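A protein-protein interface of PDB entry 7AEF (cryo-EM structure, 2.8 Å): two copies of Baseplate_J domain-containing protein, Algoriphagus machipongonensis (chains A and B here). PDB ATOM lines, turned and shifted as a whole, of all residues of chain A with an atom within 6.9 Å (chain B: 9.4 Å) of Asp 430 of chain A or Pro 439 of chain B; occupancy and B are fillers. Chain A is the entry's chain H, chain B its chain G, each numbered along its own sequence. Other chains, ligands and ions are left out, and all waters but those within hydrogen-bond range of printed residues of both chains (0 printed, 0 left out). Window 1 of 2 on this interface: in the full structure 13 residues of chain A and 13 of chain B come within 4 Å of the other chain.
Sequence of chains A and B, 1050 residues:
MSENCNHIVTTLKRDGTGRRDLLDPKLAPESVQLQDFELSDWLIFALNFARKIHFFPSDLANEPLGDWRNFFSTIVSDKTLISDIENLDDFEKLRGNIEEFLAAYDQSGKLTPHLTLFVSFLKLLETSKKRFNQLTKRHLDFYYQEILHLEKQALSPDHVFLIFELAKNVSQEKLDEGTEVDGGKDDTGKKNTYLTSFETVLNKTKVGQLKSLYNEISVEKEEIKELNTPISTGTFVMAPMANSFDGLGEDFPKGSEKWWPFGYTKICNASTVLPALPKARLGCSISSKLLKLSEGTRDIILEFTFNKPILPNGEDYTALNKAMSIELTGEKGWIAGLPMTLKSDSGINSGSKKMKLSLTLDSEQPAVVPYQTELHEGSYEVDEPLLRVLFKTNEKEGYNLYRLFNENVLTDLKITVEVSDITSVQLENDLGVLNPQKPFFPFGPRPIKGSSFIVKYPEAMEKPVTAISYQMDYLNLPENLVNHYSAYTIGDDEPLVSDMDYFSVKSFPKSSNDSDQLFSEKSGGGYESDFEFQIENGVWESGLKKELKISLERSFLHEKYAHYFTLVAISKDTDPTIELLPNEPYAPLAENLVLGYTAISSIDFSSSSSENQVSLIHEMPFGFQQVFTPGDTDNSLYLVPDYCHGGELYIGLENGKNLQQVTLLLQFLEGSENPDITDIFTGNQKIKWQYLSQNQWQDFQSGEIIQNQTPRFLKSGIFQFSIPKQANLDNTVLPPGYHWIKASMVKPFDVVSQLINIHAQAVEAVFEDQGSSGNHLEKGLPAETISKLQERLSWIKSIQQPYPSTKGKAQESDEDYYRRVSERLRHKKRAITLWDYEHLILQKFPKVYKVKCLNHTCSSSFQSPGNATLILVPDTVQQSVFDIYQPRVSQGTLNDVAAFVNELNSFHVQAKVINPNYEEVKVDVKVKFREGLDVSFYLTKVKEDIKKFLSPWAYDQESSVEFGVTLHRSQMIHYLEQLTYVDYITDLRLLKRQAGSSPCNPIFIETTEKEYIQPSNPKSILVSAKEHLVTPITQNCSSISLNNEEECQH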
ATOM      1  N   GLU A 428       6.553  16.532  -3.599  1.00  0.00           N
ATOM      2  CA  GLU A 428       7.523  17.376  -4.238  1.00  0.00           C
ATOM      3  C   GLU A 428       7.072  18.803  -4.286  1.00  0.00           C
ATOM      4  O   GLU A 428       5.905  19.093  -4.238  1.00  0.00           O
ATOM      5  CB  GLU A 428       7.657  16.976  -5.672  1.00  0.00           C
ATOM      6  CG  GLU A 428       8.508  15.780  -5.923  1.00  0.00           C
ATOM      7  CD  GLU A 428       8.651  15.556  -7.398  1.00  0.00           C
ATOM      8  OE1 GLU A 428       8.503  16.549  -8.136  1.00  0.00           O
ATOM      9  OE2 GLU A 428       8.894  14.406  -7.821  1.00  0.00           O
ATOM     10  N   ASN A 429       8.053  19.677  -4.411  1.00  0.00           N
ATOM     11  CA  ASN A 429       7.916  21.119  -4.599  1.00  0.00           C
ATOM     12  C   ASN A 429       8.995  21.540  -5.614  1.00  0.00           C
ATOM     13  O   ASN A 429       9.804  20.732  -6.041  1.00  0.00           O
ATOM     14  CB  ASN A 429       7.859  21.951  -3.302  1.00  0.00           C
ATOM     15  CG  ASN A 429       9.126  21.902  -2.499  1.00  0.00           C
ATOM     16  OD1 ASN A 429      10.123  21.403  -2.941  1.00  0.00           O
ATOM     17  ND2 ASN A 429       9.069  22.393  -1.296  1.00  0.00           N
ATOM     18  N   ASP A 430       9.048  22.798  -6.002  1.00  0.00           N
ATOM     19  CA  ASP A 430       9.985  23.196  -7.051  1.00  0.00           C
ATOM     20  C   ASP A 430      11.447  22.934  -6.772  1.00  0.00           C
ATOM     21  O   ASP A 430      12.240  22.957  -7.682  1.00  0.00           O
ATOM     22  CB  ASP A 430       9.822  24.663  -7.418  1.00  0.00           C
ATOM     23  CG  ASP A 430       8.378  25.079  -7.530  1.00  0.00           C
ATOM     24  OD1 ASP A 430       7.650  24.609  -8.434  1.00  0.00           O
ATOM     25  OD2 ASP A 430       7.970  25.908  -6.708  1.00  0.00           O
ATOM     26  N   LEU A 431      11.815  22.765  -5.520  1.00  0.00           N
ATOM     27  CA  LEU A 431      13.186  22.546  -5.149  1.00  0.00           C
ATOM     28  C   LEU A 431      13.564  21.080  -5.027  1.00  0.00           C
ATOM     29  O   LEU A 431      14.742  20.787  -4.838  1.00  0.00           O
ATOM     30  CB  LEU A 431      13.486  23.221  -3.815  1.00  0.00           C
ATOM     31  CG  LEU A 431      13.222  24.710  -3.637  1.00  0.00           C
ATOM     32  CD1 LEU A 431      13.414  25.079  -2.182  1.00  0.00           C
ATOM     33  CD2 LEU A 431      14.139  25.523  -4.525  1.00  0.00           C
ATOM     34  N   GLY A 432      12.622  20.149  -5.112  1.00  0.00           N
ATOM     35  CA  GLY A 432      13.008  18.761  -4.941  1.00  0.00           C
ATOM     36  C   GLY A 432      12.024  17.918  -4.119  1.00  0.00           C
ATOM     37  O   GLY A 432      10.853  18.251  -3.954  1.00  0.00           O
ATOM     38  N   PRO A 442       5.349  23.000   2.126  1.00  0.00           N
ATOM     39  CA  PRO A 442       4.783  22.640   0.813  1.00  0.00           C
ATOM     40  C   PRO A 442       5.159  23.492  -0.401  1.00  0.00           C
ATOM     41  O   PRO A 442       5.283  22.916  -1.471  1.00  0.00           O
ATOM     42  CB  PRO A 442       3.271  22.661   1.061  1.00  0.00           C
ATOM     43  CG  PRO A 442       3.064  23.291   2.372  1.00  0.00           C
ATOM     44  CD  PRO A 442       4.316  23.163   3.154  1.00  0.00           C
ATOM     45  N   PHE A 443       5.316  24.811  -0.288  1.00  0.00           N
ATOM     46  CA  PHE A 443       5.688  25.685  -1.400  1.00  0.00           C
ATOM     47  C   PHE A 443       7.058  26.288  -1.184  1.00  0.00           C
ATOM     48  O   PHE A 443       7.359  27.349  -1.709  1.00  0.00           O
ATOM     49  CB  PHE A 443       4.677  26.818  -1.563  1.00  0.00           C
ATOM     50  CG  PHE A 443       3.268  26.360  -1.617  1.00  0.00           C
ATOM     51  CD1 PHE A 443       2.730  25.893  -2.795  1.00  0.00           C
ATOM     52  CD2 PHE A 443       2.482  26.374  -0.487  1.00  0.00           C
ATOM     53  CE1 PHE A 443       1.433  25.464  -2.847  1.00  0.00           C
ATOM     54  CE2 PHE A 443       1.186  25.942  -0.534  1.00  0.00           C
ATOM     55  CZ  PHE A 443       0.661  25.485  -1.718  1.00  0.00           C
ATOM     56  N   GLY A 444       7.883  25.638  -0.398  1.00  0.00           N
ATOM     57  CA  GLY A 444       9.155  26.195  -0.001  1.00  0.00           C
ATOM     58  C   GLY A 444       9.162  26.958   1.323  1.00  0.00           C
ATOM     59  O   GLY A 444       8.124  27.381   1.828  1.00  0.00           O
ATOM     60  N   ILE A 448       6.433  32.271  -3.702  1.00  0.00           N
ATOM     61  CA  ILE A 448       6.261  33.312  -4.705  1.00  0.00           C
ATOM     62  C   ILE A 448       5.029  33.000  -5.531  1.00  0.00           C
ATOM     63  O   ILE A 448       4.551  31.866  -5.550  1.00  0.00           O
ATOM     64  CB  ILE A 448       7.479  33.417  -5.628  1.00  0.00           C
ATOM     65  CG1 ILE A 448       7.657  32.097  -6.398  1.00  0.00           C
ATOM     66  CG2 ILE A 448       8.703  33.754  -4.812  1.00  0.00           C
ATOM     67  CD1 ILE A 448       8.681  32.126  -7.487  1.00  0.00           C
ATOM     68  N   GLY A 450       2.869  31.800  -8.326  1.00  0.00           N
ATOM     69  CA  GLY A 450       3.102  30.742  -9.274  1.00  0.00           C
ATOM     70  C   GLY A 450       3.811  29.514  -8.744  1.00  0.00           C
ATOM     71  O   GLY A 450       3.938  28.541  -9.497  1.00  0.00           O
ATOM     72  N   SER A 451       4.267  29.500  -7.481  1.00  0.00           N
ATOM     73  CA  SER A 451       4.978  28.308  -7.031  1.00  0.00           C
ATOM     74  C   SER A 451       3.957  27.206  -6.806  1.00  0.00           C
ATOM     75  O   SER A 451       2.751  27.468  -6.729  1.00  0.00           O
ATOM     76  CB  SER A 451       5.722  28.472  -5.705  1.00  0.00           C
ATOM     77  OG  SER A 451       4.901  28.923  -4.663  1.00  0.00           O
ATOM     78  N   SER A 452       4.420  25.961  -6.658  1.00  0.00           N
ATOM     79  CA  SER A 452       3.453  24.871  -6.603  1.00  0.00           C
ATOM     80  C   SER A 452       3.817  23.780  -5.601  1.00  0.00           C
ATOM     81  O   SER A 452       4.922  23.729  -5.053  1.00  0.00           O
ATOM     82  CB  SER A 452       3.303  24.135  -7.921  1.00  0.00           C
ATOM     83  OG  SER A 452       4.538  23.628  -8.364  1.00  0.00           O
ATOM     84  N   PHE A 453       2.865  22.860  -5.423  1.00  0.00           N
ATOM     85  CA  PHE A 453       3.003  21.681  -4.571  1.00  0.00           C
ATOM     86  C   PHE A 453       2.327  20.475  -5.214  1.00  0.00           C
ATOM     87  O   PHE A 453       1.156  20.542  -5.603  1.00  0.00           O
ATOM     88  CB  PHE A 453       2.407  21.954  -3.195  1.00  0.00           C
ATOM     89  CG  PHE A 453       2.422  20.781  -2.269  1.00  0.00           C
ATOM     90  CD1 PHE A 453       3.607  20.220  -1.837  1.00  0.00           C
ATOM     91  CD2 PHE A 453       1.239  20.265  -1.797  1.00  0.00           C
ATOM     92  CE1 PHE A 453       3.594  19.163  -0.962  1.00  0.00           C
ATOM     93  CE2 PHE A 453       1.231  19.211  -0.929  1.00  0.00           C
ATOM     94  CZ  PHE A 453       2.407  18.664  -0.513  1.00  0.00           C
ATOM     95  N   ILE A 454       3.059  19.365  -5.329  1.00  0.00           N
ATOM     96  CA  ILE A 454       2.575  18.183  -6.044  1.00  0.00           C
ATOM     97  C   ILE A 454       2.572  16.918  -5.179  1.00  0.00           C
ATOM     98  O   ILE A 454       3.585  16.565  -4.567  1.00  0.00           O
ATOM     99  CB  ILE A 454       3.384  17.946  -7.323  1.00  0.00           C
ATOM    100  CG1 ILE A 454       3.166  19.126  -8.263  1.00  0.00           C
ATOM    101  CG2 ILE A 454       2.955  16.655  -7.994  1.00  0.00           C
ATOM    102  CD1 ILE A 454       4.037  19.141  -9.458  1.00  0.00           C
ATOM    103  N   LEU B 427      19.068  21.492 -22.220  1.00  0.00           N
ATOM    104  CA  LEU B 427      19.086  22.934 -22.011  1.00  0.00           C
ATOM    105  C   LEU B 427      20.350  23.388 -21.318  1.00  0.00           C
ATOM    106  O   LEU B 427      20.804  22.756 -20.359  1.00  0.00           O
ATOM    107  CB  LEU B 427      17.916  23.384 -21.180  1.00  0.00           C
ATOM    108  CG  LEU B 427      16.575  23.015 -21.752  1.00  0.00           C
ATOM    109  CD1 LEU B 427      15.521  23.562 -20.830  1.00  0.00           C
ATOM    110  CD2 LEU B 427      16.505  23.601 -23.125  1.00  0.00           C
ATOM    111  N   ASN B 429      22.861  26.928 -19.982  1.00  0.00           N
ATOM    112  CA  ASN B 429      23.194  28.262 -19.520  1.00  0.00           C
ATOM    113  C   ASN B 429      24.662  28.543 -19.721  1.00  0.00           C
ATOM    114  O   ASN B 429      25.459  27.647 -19.973  1.00  0.00           O
ATOM    115  CB  ASN B 429      22.945  28.425 -18.023  1.00  0.00           C
ATOM    116  CG  ASN B 429      21.713  29.140 -17.732  1.00  0.00           C
ATOM    117  OD1 ASN B 429      21.252  29.910 -18.554  1.00  0.00           O
ATOM    118  ND2 ASN B 429      21.272  29.071 -16.498  1.00  0.00           N
ATOM    119  N   LEU B 434      21.016  22.754 -17.268  1.00  0.00           N
ATOM    120  CA  LEU B 434      19.802  23.090 -16.569  1.00  0.00           C
ATOM    121  C   LEU B 434      19.005  21.808 -16.403  1.00  0.00           C
ATOM    122  O   LEU B 434      19.189  20.854 -17.157  1.00  0.00           O
ATOM    123  CB  LEU B 434      19.030  24.142 -17.359  1.00  0.00           C
ATOM    124  CG  LEU B 434      19.852  25.385 -17.705  1.00  0.00           C
ATOM    125  CD1 LEU B 434      19.081  26.349 -18.566  1.00  0.00           C
ATOM    126  CD2 LEU B 434      20.265  26.034 -16.432  1.00  0.00           C
ATOM    127  N   ASN B 435      18.167  21.762 -15.385  1.00  0.00           N
ATOM    128  CA  ASN B 435      17.317  20.605 -15.184  1.00  0.00           C
ATOM    129  C   ASN B 435      15.953  20.973 -15.741  1.00  0.00           C
ATOM    130  O   ASN B 435      15.285  21.847 -15.178  1.00  0.00           O
ATOM    131  CB  ASN B 435      17.248  20.256 -13.698  1.00  0.00           C
ATOM    132  CG  ASN B 435      16.462  18.991 -13.391  1.00  0.00           C
ATOM    133  OD1 ASN B 435      15.800  18.408 -14.238  1.00  0.00           O
ATOM    134  ND2 ASN B 435      16.524  18.575 -12.143  1.00  0.00           N
ATOM    135  N   PRO B 436      15.514  20.346 -16.838  1.00  0.00           N
ATOM    136  CA  PRO B 436      14.251  20.731 -17.491  1.00  0.00           C
ATOM    137  C   PRO B 436      12.994  20.403 -16.706  1.00  0.00           C
ATOM    138  O   PRO B 436      11.948  21.007 -16.972  1.00  0.00           O
ATOM    139  CB  PRO B 436      14.296  19.937 -18.806  1.00  0.00           C
ATOM    140  CG  PRO B 436      15.727  19.639 -19.016  1.00  0.00           C
ATOM    141  CD  PRO B 436      16.287  19.412 -17.663  1.00  0.00           C
ATOM    142  N   GLN B 437      13.058  19.479 -15.753  1.00  0.00           N
ATOM    143  CA  GLN B 437      11.860  19.095 -15.031  1.00  0.00           C
ATOM    144  C   GLN B 437      11.329  20.174 -14.112  1.00  0.00           C
ATOM    145  O   GLN B 437      10.112  20.296 -13.929  1.00  0.00           O
ATOM    146  CB  GLN B 437      12.117  17.821 -14.228  1.00  0.00           C
ATOM    147  CG  GLN B 437      12.490  16.561 -15.005  1.00  0.00           C
ATOM    148  CD  GLN B 437      11.475  16.105 -16.076  1.00  0.00           C
ATOM    149  OE1 GLN B 437      11.792  15.228 -16.857  1.00  0.00           O
ATOM    150  NE2 GLN B 437      10.291  16.711 -16.151  1.00  0.00           N
ATOM    151  N   LYS B 438      12.214  20.956 -13.547  1.00  0.00           N
ATOM    152  CA  LYS B 438      11.921  21.931 -12.526  1.00  0.00           C
ATOM    153  C   LYS B 438      12.029  23.334 -13.107  1.00  0.00           C
ATOM    154  O   LYS B 438      12.497  23.509 -14.237  1.00  0.00           O
ATOM    155  CB  LYS B 438      12.907  21.730 -11.366  1.00  0.00           C
ATOM    156  CG  LYS B 438      12.821  20.386 -10.698  1.00  0.00           C
ATOM    157  CD  LYS B 438      11.558  20.281  -9.898  1.00  0.00           C
ATOM    158  CE  LYS B 438      11.430  18.967  -9.175  1.00  0.00           C
ATOM    159  NZ  LYS B 438      10.117  18.956  -8.478  1.00  0.00           N
ATOM    160  N   PRO B 439      11.545  24.356 -12.387  1.00  0.00           N
ATOM    161  CA  PRO B 439      11.739  25.744 -12.825  1.00  0.00           C
ATOM    162  C   PRO B 439      13.214  26.112 -12.866  1.00  0.00           C
ATOM    163  O   PRO B 439      13.976  25.781 -11.960  1.00  0.00           O
ATOM    164  CB  PRO B 439      10.987  26.546 -11.758  1.00  0.00           C
ATOM    165  CG  PRO B 439       9.968  25.596 -11.243  1.00  0.00           C
ATOM    166  CD  PRO B 439      10.577  24.276 -11.276  1.00  0.00           C
ATOM    167  N   PHE B 440      13.623  26.778 -13.941  1.00  0.00           N
ATOM    168  CA  PHE B 440      15.031  27.063 -14.181  1.00  0.00           C
ATOM    169  C   PHE B 440      15.192  28.508 -14.618  1.00  0.00           C
ATOM    170  O   PHE B 440      14.233  29.142 -15.051  1.00  0.00           O
ATOM    171  CB  PHE B 440      15.618  26.131 -15.245  1.00  0.00           C
ATOM    172  CG  PHE B 440      14.896  26.176 -16.560  1.00  0.00           C
ATOM    173  CD1 PHE B 440      15.295  27.040 -17.567  1.00  0.00           C
ATOM    174  CD2 PHE B 440      13.827  25.335 -16.794  1.00  0.00           C
ATOM    175  CE1 PHE B 440      14.625  27.076 -18.743  1.00  0.00           C
ATOM    176  CE2 PHE B 440      13.162  25.367 -17.972  1.00  0.00           C
ATOM    177  CZ  PHE B 440      13.564  26.224 -18.942  1.00  0.00           C
ATOM    178  N   PHE B 441      16.409  29.029 -14.492  1.00  0.00           N
ATOM    179  CA  PHE B 441      16.701  30.386 -14.937  1.00  0.00           C
ATOM    180  C   PHE B 441      17.367  30.339 -16.283  1.00  0.00           C
ATOM    181  O   PHE B 441      18.589  30.142 -16.341  1.00  0.00           O
ATOM    182  CB  PHE B 441      17.624  31.103 -13.962  1.00  0.00           C
ATOM    183  CG  PHE B 441      17.006  31.490 -12.700  1.00  0.00           C
ATOM    184  CD1 PHE B 441      16.165  32.578 -12.628  1.00  0.00           C
ATOM    185  CD2 PHE B 441      17.329  30.808 -11.555  1.00  0.00           C
ATOM    186  CE1 PHE B 441      15.626  32.948 -11.433  1.00  0.00           C
ATOM    187  CE2 PHE B 441      16.796  31.173 -10.361  1.00  0.00           C
ATOM    188  CZ  PHE B 441      15.941  32.245 -10.298  1.00  0.00           C
ATOM    189  N   PRO B 442      16.657  30.587 -17.381  1.00  0.00           N
ATOM    190  CA  PRO B 442      17.349  30.908 -18.622  1.00  0.00           C
ATOM    191  C   PRO B 442      18.064  32.217 -18.383  1.00  0.00           C
ATOM    192  O   PRO B 442      17.605  33.040 -17.582  1.00  0.00           O
ATOM    193  CB  PRO B 442      16.213  31.044 -19.637  1.00  0.00           C
ATOM    194  CG  PRO B 442      15.063  31.488 -18.834  1.00  0.00           C
ATOM    195  CD  PRO B 442      15.219  30.847 -17.496  1.00  0.00           C
ATOM    196  N   MET B 472       7.733  28.475 -24.062  1.00  0.00           N
ATOM    197  CA  MET B 472       8.024  28.494 -22.618  1.00  0.00           C
ATOM    198  C   MET B 472       7.026  29.342 -21.832  1.00  0.00           C
ATOM    199  O   MET B 472       6.508  30.328 -22.347  1.00  0.00           O
ATOM    200  CB  MET B 472       9.386  29.104 -22.287  1.00  0.00           C
ATOM    201  CG  MET B 472      10.546  28.539 -22.974  1.00  0.00           C
ATOM    202  SD  MET B 472      12.055  29.412 -22.624  1.00  0.00           S
ATOM    203  CE  MET B 472      12.454  28.674 -21.087  1.00  0.00           C
ATOM    204  N   ASP B 473       6.834  29.021 -20.542  1.00  0.00           N
ATOM    205  CA  ASP B 473       6.041  29.826 -19.605  1.00  0.00           C
ATOM    206  C   ASP B 473       6.928  30.492 -18.552  1.00  0.00           C
ATOM    207  O   ASP B 473       7.923  29.916 -18.125  1.00  0.00           O
ATOM    208  CB  ASP B 473       5.014  28.974 -18.844  1.00  0.00           C
ATOM    209  CG  ASP B 473       3.874  28.479 -19.707  1.00  0.00           C
ATOM    210  OD1 ASP B 473       3.413  29.215 -20.599  1.00  0.00           O
ATOM    211  OD2 ASP B 473       3.418  27.342 -19.466  1.00  0.00           O
ATOM    212  N   TYR B 474       6.535  31.675 -18.067  1.00  0.00           N
ATOM    213  CA  TYR B 474       7.243  32.326 -16.964  1.00  0.00           C
ATOM    214  C   TYR B 474       6.452  32.213 -15.663  1.00  0.00           C
ATOM    215  O   TYR B 474       5.230  32.077 -15.688  1.00  0.00           O
ATOM    216  CB  TYR B 474       7.519  33.789 -17.290  1.00  0.00           C
ATOM    217  CG  TYR B 474       8.505  33.902 -18.396  1.00  0.00           C
ATOM    218  CD1 TYR B 474       9.851  33.692 -18.160  1.00  0.00           C
ATOM    219  CD2 TYR B 474       8.092  34.169 -19.686  1.00  0.00           C
ATOM    220  CE1 TYR B 474      10.758  33.772 -19.167  1.00  0.00           C
ATOM    221  CE2 TYR B 474       8.995  34.250 -20.704  1.00  0.00           C
ATOM    222  CZ  TYR B 474      10.325  34.048 -20.438  1.00  0.00           C
ATOM    223  OH  TYR B 474      11.240  34.128 -21.449  1.00  0.00           O
ATOM    224  N   LEU B 475       7.144  32.281 -14.515  1.00  0.00           N
ATOM    225  CA  LEU B 475       6.514  31.927 -13.235  1.00  0.00           C
ATOM    226  C   LEU B 475       6.004  33.094 -12.395  1.00  0.00           C
ATOM    227  O   LEU B 475       4.824  33.114 -12.038  1.00  0.00           O
ATOM    228  CB  LEU B 475       7.440  31.104 -12.342  1.00  0.00           C
ATOM    229  CG  LEU B 475       7.377  29.596 -12.484  1.00  0.00           C
ATOM    230  CD1 LEU B 475       8.147  29.230 -13.680  1.00  0.00           C
ATOM    231  CD2 LEU B 475       7.970  28.954 -11.268  1.00  0.00           C
ATOM    232  N   ASN B 476       6.857  34.024 -11.982  1.00  0.00           N
ATOM    233  CA  ASN B 476       6.363  35.085 -11.095  1.00  0.00           C
ATOM    234  C   ASN B 476       6.693  36.452 -11.689  1.00  0.00           C
ATOM    235  O   ASN B 476       7.419  37.292 -11.166  1.00  0.00           O
ATOM    236  CB  ASN B 476       6.779  34.911  -9.634  1.00  0.00           C
ATOM    237  CG  ASN B 476       8.215  35.212  -9.368  1.00  0.00           C
ATOM    238  OD1 ASN B 476       9.094  34.754 -10.078  1.00  0.00           O
ATOM    239  ND2 ASN B 476       8.459  36.054  -8.376  1.00  0.00           N
ATOM    240  N   PRO B 588      14.257  36.111 -15.046  1.00  0.00           N
ATOM    241  CA  PRO B 588      13.192  35.383 -15.762  1.00  0.00           C
ATOM    242  C   PRO B 588      13.175  33.872 -15.632  1.00  0.00           C
ATOM    243  O   PRO B 588      13.378  33.179 -16.587  1.00  0.00           O
ATOM    244  CB  PRO B 588      13.408  35.843 -17.207  1.00  0.00           C
ATOM    245  CG  PRO B 588      14.836  36.109 -17.281  1.00  0.00           C
ATOM    246  CD  PRO B 588      15.212  36.710 -15.984  1.00  0.00           C
ATOM    247  N   LEU B 589      12.825  33.397 -14.440  1.00  0.00           N
ATOM    248  CA  LEU B 589      12.666  31.974 -14.146  1.00  0.00           C
ATOM    249  C   LEU B 589      11.534  31.338 -14.955  1.00  0.00           C
ATOM    250  O   LEU B 589      10.443  31.899 -15.042  1.00  0.00           O
ATOM    251  CB  LEU B 589      12.380  31.836 -12.653  1.00  0.00           C
ATOM    252  CG  LEU B 589      12.240  30.473 -12.001  1.00  0.00           C
ATOM    253  CD1 LEU B 589      13.555  29.794 -11.944  1.00  0.00           C
ATOM    254  CD2 LEU B 589      11.735  30.663 -10.604  1.00  0.00           C
ATOM    255  N   ALA B 590      11.765  30.138 -15.516  1.00  0.00           N
ATOM    256  CA  ALA B 590      10.810  29.556 -16.469  1.00  0.00           C
ATOM    257  C   ALA B 590      10.673  28.034 -16.367  1.00  0.00           C
ATOM    258  O   ALA B 590      11.476  27.357 -15.726  1.00  0.00           O
ATOM    259  CB  ALA B 590      11.200  29.910 -17.900  1.00  0.00           C
ATOM    260  N   GLU B 591       9.669  27.494 -17.082  1.00  0.00           N
ATOM    261  CA  GLU B 591       9.365  26.057 -17.091  1.00  0.00           C
ATOM    262  C   GLU B 591       8.504  25.644 -18.298  1.00  0.00           C
ATOM    263  O   GLU B 591       7.929  26.484 -18.988  1.00  0.00           O
ATOM    264  CB  GLU B 591       8.651  25.676 -15.811  1.00  0.00           C
ATOM    265  CG  GLU B 591       7.386  26.438 -15.679  1.00  0.00           C
ATOM    266  CD  GLU B 591       6.435  25.788 -14.749  1.00  0.00           C
ATOM    267  OE1 GLU B 591       6.899  25.050 -13.856  1.00  0.00           O
ATOM    268  OE2 GLU B 591       5.222  25.992 -14.928  1.00  0.00           O
ATOM    269  N   ASN B 592       8.436  24.314 -18.538  1.00  0.00           N
ATOM    270  CA  ASN B 592       7.602  23.603 -19.556  1.00  0.00           C
ATOM    271  C   ASN B 592       7.908  23.897 -21.044  1.00  0.00           C
ATOM    272  O   ASN B 592       7.001  24.199 -21.817  1.00  0.00           O
ATOM    273  CB  ASN B 592       6.110  23.849 -19.321  1.00  0.00           C
ATOM    274  CG  ASN B 592       5.583  23.134 -18.117  1.00  0.00           C
ATOM    275  OD1 ASN B 592       6.258  22.299 -17.527  1.00  0.00           O
ATOM    276  ND2 ASN B 592       4.362  23.467 -17.732  1.00  0.00           N
ATOM    277  N   LEU B 593       9.151  23.686 -21.473  1.00  0.00           N
ATOM    278  CA  LEU B 593       9.537  23.885 -22.879  1.00  0.00           C
ATOM    279  C   LEU B 593       9.057  22.775 -23.846  1.00  0.00           C
ATOM    280  O   LEU B 593       9.139  21.594 -23.517  1.00  0.00           O
ATOM    281  CB  LEU B 593      11.056  23.993 -22.930  1.00  0.00           C
ATOM    282  CG  LEU B 593      11.712  24.226 -24.263  1.00  0.00           C
ATOM    283  CD1 LEU B 593      11.277  25.464 -24.563  1.00  0.00           C
ATOM    284  CD2 LEU B 593      13.156  24.301 -24.093  1.00  0.00           C
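The backbone carbonyl oxygen of Asn 429 of chain A is in hydrogen-bond range of the side-chain amino group of Lys 438 of chain B (3.0 Å). OE1 of Glu 428 of chain A lies within salt-bridge range of NZ of Lys 438 of chain B (2.9 Å).
O of Ile 448 of chain A sits at hydrogen-bond distance from OG of Ser 451 of chain A (3.1 Å). The side-chain carboxylate (OD1) of Asp 430 of chain A sits at hydrogen-bond distance from the side-chain hydroxyl (OG) of Ser 452 of chain A, at 3.3 Å. The backbone carbonyl oxygen (O) of Gly 432 of chain A lies close to the side-chain amide oxygen (OD1) of Asn 429 of chain A, 3.4 Å away. OD1 of Asn 429 of chain A lies close to N of Leu 431 of chain A (3.4 Å). The backbone NH (N) of Ile 454 of chain A lies within hydrogen-bond range of the backbone carbonyl oxygen (O) of Glu 428 of chain A.
Lys 438 of chain B touches Asp 430 of chain A (CD to O, 3.5 Å). CG of Pro 439 of chain B touches OD1 of Asp 430 of chain A, 3.8 Å away. Asn 476 of chain B touches Ile 448 of chain A (CG to CD1, 3.6 Å).
Of chain B, only Lys 438 (3.5 Å) and Pro 439 (3.8 Å) come within 4 Å of Asp 430 of chain A. Printed residues of chain B within 4 Å of Ile 448 of chain A: Asn 476. Leu 434 of chain B touches none of the printed residues of chain A. Of the printed residues of chain A, Asn 476 of chain B touches Ile 448 (3.6 Å). The nearest residue of chain B that does not touch Asp 430 of chain A is Leu 475 of chain B (5.2 Å). The nearest printed residue of chain B that does not touch Glu 428 of chain A is Gln 437 of chain B (7.1 Å).
Of the 14 printed residues of chain A, 4 touch a printed residue of chain B. Hydrophobic or aromatic side chains of chain A that line the printed part of chain B: Ile 448. Printed residues of chain B that touch a printed residue of chain A: Lys 438, Pro 439 and Asn 476. Hydrophobic or aromatic side chains of chain B within 4 Å of the printed part of chain A: Pro 439. Among the printed residues, 5 pairs touch across the chains. Among the printed residues, Asp or Glu carboxylates within 4 Å of a Lys or Arg side-chain nitrogen of the other chain: Glu 428 of chain A with Lys 438 of chain B.
Positions printed for both chains: 429 and 442. Of the 5 pairs that touch across the chains among the printed residues, none has its exchanged pair printed and touching as well.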
